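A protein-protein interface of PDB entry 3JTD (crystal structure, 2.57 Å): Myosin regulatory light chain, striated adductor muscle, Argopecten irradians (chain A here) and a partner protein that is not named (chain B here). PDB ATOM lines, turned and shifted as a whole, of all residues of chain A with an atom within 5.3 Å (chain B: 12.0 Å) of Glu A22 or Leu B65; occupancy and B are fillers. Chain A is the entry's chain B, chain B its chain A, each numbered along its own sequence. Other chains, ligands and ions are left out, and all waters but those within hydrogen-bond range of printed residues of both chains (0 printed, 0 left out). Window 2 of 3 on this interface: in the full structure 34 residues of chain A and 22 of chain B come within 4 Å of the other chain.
CB of Glu A19 touches OH of Tyr B58, at 3.9 Å. Glu A19 touches Lys B62 (OE1 to CG, 3.8 Å). Met A20 touches Tyr B58. Glu A22 touches Leu B65 (O to CD2, 3.6 Å). CE1 of Tyr B58 touches CB of Ala A23 (3.5 Å). Ala A23 touches Leu B65. CG1 of Val B61 touches SD of Met A26 (3.9 Å). CD1 of Leu B64 touches SD of Met A26, at 3.3 Å.
Of the printed residues of chain B, Glu A22 touches Leu B65. Gln A18 touches none of the printed residues of chain B. Glu A19 touches just these residues of chain B: Tyr B58 (3.9 Å) and Lys B62 (3.8 Å). Of chain B, only Tyr B58 and Leu B65 come within 4 Å of Ala A23. No residue of chain B comes within 4 Å of Ser A25. Printed residues of chain B within 4 Å of Met A26: Val B61 and Leu B64. Of the printed residues of chain B, Met A20 touches Tyr B58 (3.4 Å). Of the printed residues of chain A, Tyr B58 touches Glu A19, Met A20 and Ala A23. Printed residues of chain A within 4 Å of Leu B64: Met A26 (3.3 Å). Printed residues of chain A within 4 Å of Lys B62: Glu A19. Of the printed residues of chain A, Val B61 touches Met A26 (3.9 Å). The nearest residue of chain B that does not touch Glu A22 is Val B61 (6.0 Å). The nearest residue of chain A that does not touch Leu B65 is Met A26 (4.2 Å). The nearest printed residue of chain A that does not touch Lys B62 is Ala A23 (6.2 Å).
Hydrophobic or aromatic side chains of chain B that line the printed part of chain A: Tyr B58, Val B61, Leu B64 and Leu B65. Hydrophobic or aromatic side chains of chain A that line the printed part of chain B: Met A20, Ala A23 and Met A26. Among the printed residues, no Asp or Glu carboxylate lies within 4 Å of a Lys or Arg side-chain nitrogen of the other chain.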
ATOM      1  N   GLN A  18      12.477 -15.625 -26.470  1.00  0.00           N
ATOM      2  CA  GLN A  18      12.926 -15.566 -27.857  1.00  0.00           C
ATOM      3  C   GLN A  18      12.734 -14.144 -28.392  1.00  0.00           C
ATOM      4  O   GLN A  18      13.571 -13.636 -29.142  1.00  0.00           O
ATOM      5  CB  GLN A  18      12.152 -16.554 -28.732  1.00  0.00           C
ATOM      6  CG  GLN A  18      12.794 -16.776 -30.103  1.00  0.00           C
ATOM      7  CD  GLN A  18      14.148 -17.478 -30.006  1.00  0.00           C
ATOM      8  OE1 GLN A  18      14.616 -17.806 -28.913  1.00  0.00           O
ATOM      9  NE2 GLN A  18      14.780 -17.711 -31.152  1.00  0.00           N
ATOM     10  N   GLU A  19      11.626 -13.513 -28.000  1.00  0.00           N
ATOM     11  CA  GLU A  19      11.322 -12.142 -28.412  1.00  0.00           C
ATOM     12  C   GLU A  19      12.423 -11.204 -27.959  1.00  0.00           C
ATOM     13  O   GLU A  19      12.979 -10.438 -28.754  1.00  0.00           O
ATOM     14  CB  GLU A  19      10.005 -11.661 -27.795  1.00  0.00           C
ATOM     15  CG  GLU A  19       8.759 -12.031 -28.574  1.00  0.00           C
ATOM     16  CD  GLU A  19       7.602 -11.083 -28.284  1.00  0.00           C
ATOM     17  OE1 GLU A  19       7.784  -9.863 -28.487  1.00  0.00           O
ATOM     18  OE2 GLU A  19       6.517 -11.555 -27.858  1.00  0.00           O
ATOM     19  N   MET A  20      12.708 -11.274 -26.664  1.00  0.00           N
ATOM     20  CA  MET A  20      13.728 -10.464 -26.022  1.00  0.00           C
ATOM     21  C   MET A  20      15.107 -10.477 -26.673  1.00  0.00           C
ATOM     22  O   MET A  20      15.819  -9.466 -26.625  1.00  0.00           O
ATOM     23  CB  MET A  20      13.853 -10.870 -24.559  1.00  0.00           C
ATOM     24  CG  MET A  20      12.588 -10.624 -23.803  1.00  0.00           C
ATOM     25  SD  MET A  20      12.518 -11.590 -22.317  1.00  0.00           S
ATOM     26  CE  MET A  20      12.520 -10.304 -21.047  1.00  0.00           C
ATOM     27  N   LYS A  21      15.514 -11.592 -27.271  1.00  0.00           N
ATOM     28  CA  LYS A  21      16.828 -11.573 -27.901  1.00  0.00           C
ATOM     29  C   LYS A  21      16.755 -10.787 -29.214  1.00  0.00           C
ATOM     30  O   LYS A  21      17.724 -10.159 -29.633  1.00  0.00           O
ATOM     31  CB  LYS A  21      17.386 -12.991 -28.102  1.00  0.00           C
ATOM     32  CG  LYS A  21      16.784 -13.837 -29.205  1.00  0.00           C
ATOM     33  CD  LYS A  21      17.588 -15.142 -29.306  1.00  0.00           C
ATOM     34  CE  LYS A  21      17.208 -15.980 -30.518  1.00  0.00           C
ATOM     35  NZ  LYS A  21      18.073 -17.195 -30.665  1.00  0.00           N
ATOM     36  N   GLU A  22      15.584 -10.794 -29.833  1.00  0.00           N
ATOM     37  CA  GLU A  22      15.368 -10.051 -31.063  1.00  0.00           C
ATOM     38  C   GLU A  22      15.390  -8.555 -30.688  1.00  0.00           C
ATOM     39  O   GLU A  22      15.885  -7.710 -31.439  1.00  0.00           O
ATOM     40  CB  GLU A  22      14.020 -10.456 -31.666  1.00  0.00           C
ATOM     41  CG  GLU A  22      13.999 -11.885 -32.203  1.00  0.00           C
ATOM     42  CD  GLU A  22      12.591 -12.445 -32.371  1.00  0.00           C
ATOM     43  OE1 GLU A  22      11.849 -12.506 -31.362  1.00  0.00           O
ATOM     44  OE2 GLU A  22      12.230 -12.832 -33.507  1.00  0.00           O
ATOM     45  N   ALA A  23      14.859  -8.252 -29.507  1.00  0.00           N
ATOM     46  CA  ALA A  23      14.843  -6.890 -28.993  1.00  0.00           C
ATOM     47  C   ALA A  23      16.270  -6.445 -28.634  1.00  0.00           C
ATOM     48  O   ALA A  23      16.705  -5.369 -29.033  1.00  0.00           O
ATOM     49  CB  ALA A  23      13.940  -6.810 -27.749  1.00  0.00           C
ATOM     50  N   PHE A  24      16.976  -7.289 -27.879  1.00  0.00           N
ATOM     51  CA  PHE A  24      18.341  -7.018 -27.431  1.00  0.00           C
ATOM     52  C   PHE A  24      19.280  -6.737 -28.586  1.00  0.00           C
ATOM     53  O   PHE A  24      20.067  -5.789 -28.536  1.00  0.00           O
ATOM     54  CB  PHE A  24      18.901  -8.210 -26.631  1.00  0.00           C
ATOM     55  CG  PHE A  24      20.324  -8.009 -26.137  1.00  0.00           C
ATOM     56  CD1 PHE A  24      20.574  -7.402 -24.908  1.00  0.00           C
ATOM     57  CD2 PHE A  24      21.413  -8.412 -26.913  1.00  0.00           C
ATOM     58  CE1 PHE A  24      21.889  -7.197 -24.456  1.00  0.00           C
ATOM     59  CE2 PHE A  24      22.731  -8.211 -26.472  1.00  0.00           C
ATOM     60  CZ  PHE A  24      22.974  -7.601 -25.240  1.00  0.00           C
ATOM     61  N   SER A  25      19.221  -7.570 -29.615  1.00  0.00           N
ATOM     62  CA  SER A  25      20.123  -7.357 -30.725  1.00  0.00           C
ATOM     63  C   SER A  25      19.814  -6.087 -31.475  1.00  0.00           C
ATOM     64  O   SER A  25      20.718  -5.501 -32.072  1.00  0.00           O
ATOM     65  CB  SER A  25      20.177  -8.571 -31.692  1.00  0.00           C
ATOM     66  OG  SER A  25      19.047  -9.425 -31.616  1.00  0.00           O
ATOM     67  N   MET A  26      18.558  -5.642 -31.440  1.00  0.00           N
ATOM     68  CA  MET A  26      18.212  -4.404 -32.129  1.00  0.00           C
ATOM     69  C   MET A  26      18.715  -3.210 -31.318  1.00  0.00           C
ATOM     70  O   MET A  26      18.976  -2.141 -31.861  1.00  0.00           O
ATOM     71  CB  MET A  26      16.705  -4.280 -32.338  1.00  0.00           C
ATOM     72  CG  MET A  26      16.323  -2.979 -33.059  1.00  0.00           C
ATOM     73  SD  MET A  26      14.597  -2.855 -33.563  1.00  0.00           S
ATOM     74  CE  MET A  26      14.637  -3.775 -35.094  1.00  0.00           C
ATOM     75  N   TRP B  54      13.641   0.752 -18.800  1.00  0.00           N
ATOM     76  CA  TRP B  54      13.904  -0.419 -19.640  1.00  0.00           C
ATOM     77  C   TRP B  54      12.607  -0.987 -20.240  1.00  0.00           C
ATOM     78  O   TRP B  54      12.605  -1.515 -21.357  1.00  0.00           O
ATOM     79  CB  TRP B  54      14.647  -1.521 -18.853  1.00  0.00           C
ATOM     80  CG  TRP B  54      16.108  -1.198 -18.599  1.00  0.00           C
ATOM     81  CD1 TRP B  54      16.645  -0.660 -17.458  1.00  0.00           C
ATOM     82  CD2 TRP B  54      17.196  -1.350 -19.522  1.00  0.00           C
ATOM     83  NE1 TRP B  54      17.997  -0.471 -17.615  1.00  0.00           N
ATOM     84  CE2 TRP B  54      18.365  -0.883 -18.868  1.00  0.00           C
ATOM     85  CE3 TRP B  54      17.301  -1.834 -20.834  1.00  0.00           C
ATOM     86  CZ2 TRP B  54      19.636  -0.887 -19.488  1.00  0.00           C
ATOM     87  CZ3 TRP B  54      18.569  -1.841 -21.453  1.00  0.00           C
ATOM     88  CH2 TRP B  54      19.721  -1.365 -20.770  1.00  0.00           C
ATOM     89  N   TRP B  55      11.501  -0.874 -19.498  1.00  0.00           N
ATOM     90  CA  TRP B  55      10.223  -1.367 -19.998  1.00  0.00           C
ATOM     91  C   TRP B  55       9.711  -0.436 -21.107  1.00  0.00           C
ATOM     92  O   TRP B  55       9.196  -0.898 -22.134  1.00  0.00           O
ATOM     93  CB  TRP B  55       9.192  -1.472 -18.873  1.00  0.00           C
ATOM     94  CG  TRP B  55       7.859  -1.890 -19.413  1.00  0.00           C
ATOM     95  CD1 TRP B  55       6.816  -1.064 -19.749  1.00  0.00           C
ATOM     96  CD2 TRP B  55       7.472  -3.210 -19.819  1.00  0.00           C
ATOM     97  NE1 TRP B  55       5.813  -1.788 -20.350  1.00  0.00           N
ATOM     98  CE2 TRP B  55       6.183  -3.107 -20.408  1.00  0.00           C
ATOM     99  CE3 TRP B  55       8.080  -4.473 -19.758  1.00  0.00           C
ATOM    100  CZ2 TRP B  55       5.498  -4.220 -20.923  1.00  0.00           C
ATOM    101  CZ3 TRP B  55       7.397  -5.583 -20.276  1.00  0.00           C
ATOM    102  CH2 TRP B  55       6.119  -5.444 -20.848  1.00  0.00           C
ATOM    103  N   LYS B  56       9.858   0.872 -20.893  1.00  0.00           N
ATOM    104  CA  LYS B  56       9.444   1.847 -21.885  1.00  0.00           C
ATOM    105  C   LYS B  56      10.243   1.650 -23.166  1.00  0.00           C
ATOM    106  O   LYS B  56       9.690   1.670 -24.273  1.00  0.00           O
ATOM    107  CB  LYS B  56       9.679   3.259 -21.377  1.00  0.00           C
ATOM    108  CG  LYS B  56       8.844   3.634 -20.188  1.00  0.00           C
ATOM    109  CD  LYS B  56       8.686   5.121 -20.093  1.00  0.00           C
ATOM    110  CE  LYS B  56       8.305   5.553 -18.711  1.00  0.00           C
ATOM    111  NZ  LYS B  56       9.455   5.352 -17.791  1.00  0.00           N
ATOM    112  N   LEU B  57      11.548   1.450 -23.013  1.00  0.00           N
ATOM    113  CA  LEU B  57      12.409   1.250 -24.170  1.00  0.00           C
ATOM    114  C   LEU B  57      11.999   0.011 -24.922  1.00  0.00           C
ATOM    115  O   LEU B  57      12.088  -0.046 -26.145  1.00  0.00           O
ATOM    116  CB  LEU B  57      13.874   1.118 -23.740  1.00  0.00           C
ATOM    117  CG  LEU B  57      14.903   0.637 -24.778  1.00  0.00           C
ATOM    118  CD1 LEU B  57      14.776   1.416 -26.074  1.00  0.00           C
ATOM    119  CD2 LEU B  57      16.283   0.807 -24.207  1.00  0.00           C
ATOM    120  N   TYR B  58      11.514  -0.978 -24.184  1.00  0.00           N
ATOM    121  CA  TYR B  58      11.103  -2.259 -24.745  1.00  0.00           C
ATOM    122  C   TYR B  58       9.852  -2.153 -25.620  1.00  0.00           C
ATOM    123  O   TYR B  58       9.828  -2.650 -26.742  1.00  0.00           O
ATOM    124  CB  TYR B  58      10.875  -3.264 -23.612  1.00  0.00           C
ATOM    125  CG  TYR B  58      10.708  -4.692 -24.061  1.00  0.00           C
ATOM    126  CD1 TYR B  58      11.608  -5.271 -24.934  1.00  0.00           C
ATOM    127  CD2 TYR B  58       9.650  -5.462 -23.606  1.00  0.00           C
ATOM    128  CE1 TYR B  58      11.460  -6.576 -25.346  1.00  0.00           C
ATOM    129  CE2 TYR B  58       9.494  -6.768 -24.011  1.00  0.00           C
ATOM    130  CZ  TYR B  58      10.404  -7.320 -24.883  1.00  0.00           C
ATOM    131  OH  TYR B  58      10.259  -8.621 -25.298  1.00  0.00           O
ATOM    132  N   SER B  59       8.818  -1.503 -25.096  1.00  0.00           N
ATOM    133  CA  SER B  59       7.561  -1.295 -25.821  1.00  0.00           C
ATOM    134  C   SER B  59       7.750  -0.623 -27.169  1.00  0.00           C
ATOM    135  O   SER B  59       7.249  -1.102 -28.182  1.00  0.00           O
ATOM    136  CB  SER B  59       6.604  -0.430 -25.005  1.00  0.00           C
ATOM    137  OG  SER B  59       6.085  -1.138 -23.896  1.00  0.00           O
ATOM    138  N   LYS B  60       8.467   0.498 -27.169  1.00  0.00           N
ATOM    139  CA  LYS B  60       8.708   1.263 -28.386  1.00  0.00           C
ATOM    140  C   LYS B  60       9.722   0.584 -29.304  1.00  0.00           C
ATOM    141  O   LYS B  60      10.355   1.239 -30.130  1.00  0.00           O
ATOM    142  CB  LYS B  60       9.178   2.680 -28.021  1.00  0.00           C
ATOM    143  N   VAL B  61       9.878  -0.725 -29.159  1.00  0.00           N
ATOM    144  CA  VAL B  61      10.823  -1.464 -29.988  1.00  0.00           C
ATOM    145  C   VAL B  61      10.227  -2.799 -30.447  1.00  0.00           C
ATOM    146  O   VAL B  61      10.638  -3.366 -31.458  1.00  0.00           O
ATOM    147  CB  VAL B  61      12.156  -1.734 -29.222  1.00  0.00           C
ATOM    148  CG1 VAL B  61      13.027  -2.670 -30.025  1.00  0.00           C
ATOM    149  CG2 VAL B  61      12.906  -0.423 -28.962  1.00  0.00           C
ATOM    150  N   LYS B  62       9.255  -3.292 -29.691  1.00  0.00           N
ATOM    151  CA  LYS B  62       8.596  -4.550 -30.017  1.00  0.00           C
ATOM    152  C   LYS B  62       7.916  -4.482 -31.385  1.00  0.00           C
ATOM    153  O   LYS B  62       7.915  -5.456 -32.139  1.00  0.00           O
ATOM    154  CB  LYS B  62       7.556  -4.900 -28.937  1.00  0.00           C
ATOM    155  CG  LYS B  62       6.882  -6.252 -29.141  1.00  0.00           C
ATOM    156  CD  LYS B  62       5.689  -6.454 -28.217  1.00  0.00           C
ATOM    157  CE  LYS B  62       6.100  -6.552 -26.757  1.00  0.00           C
ATOM    158  NZ  LYS B  62       4.958  -6.935 -25.866  1.00  0.00           N
ATOM    159  N   PRO B  63       7.320  -3.330 -31.719  1.00  0.00           N
ATOM    160  CA  PRO B  63       6.642  -3.165 -33.005  1.00  0.00           C
ATOM    161  C   PRO B  63       7.571  -3.414 -34.184  1.00  0.00           C
ATOM    162  O   PRO B  63       7.246  -4.164 -35.101  1.00  0.00           O
ATOM    163  CB  PRO B  63       6.168  -1.715 -32.956  1.00  0.00           C
ATOM    164  CG  PRO B  63       5.911  -1.504 -31.504  1.00  0.00           C
ATOM    165  CD  PRO B  63       7.129  -2.131 -30.884  1.00  0.00           C
ATOM    166  N   LEU B  64       8.730  -2.767 -34.147  1.00  0.00           N
ATOM    167  CA  LEU B  64       9.733  -2.885 -35.195  1.00  0.00           C
ATOM    168  C   LEU B  64      10.287  -4.311 -35.336  1.00  0.00           C
ATOM    169  O   LEU B  64      11.174  -4.571 -36.150  1.00  0.00           O
ATOM    170  CB  LEU B  64      10.861  -1.883 -34.919  1.00  0.00           C
ATOM    171  CG  LEU B  64      10.984  -1.293 -33.502  1.00  0.00           C
ATOM    172  CD1 LEU B  64      12.253  -0.467 -33.422  1.00  0.00           C
ATOM    173  CD2 LEU B  64       9.781  -0.425 -33.151  1.00  0.00           C
ATOM    174  N   LEU B  65       9.747  -5.231 -34.539  1.00  0.00           N
ATOM    175  CA  LEU B  65      10.176  -6.615 -34.586  1.00  0.00           C
ATOM    176  C   LEU B  65       9.209  -7.455 -35.407  1.00  0.00           C
ATOM    177  O   LEU B  65       9.658  -8.389 -36.112  1.00  0.00           O
ATOM    178  CB  LEU B  65      10.303  -7.187 -33.172  1.00  0.00           C
ATOM    179  CG  LEU B  65      11.386  -6.568 -32.286  1.00  0.00           C
ATOM    180  CD1 LEU B  65      11.303  -7.123 -30.872  1.00  0.00           C
ATOM    181  CD2 LEU B  65      12.766  -6.800 -32.878  1.00  0.00           C
ATOM    182  OXT LEU B  65       7.987  -7.194 -35.334  1.00  0.00           O
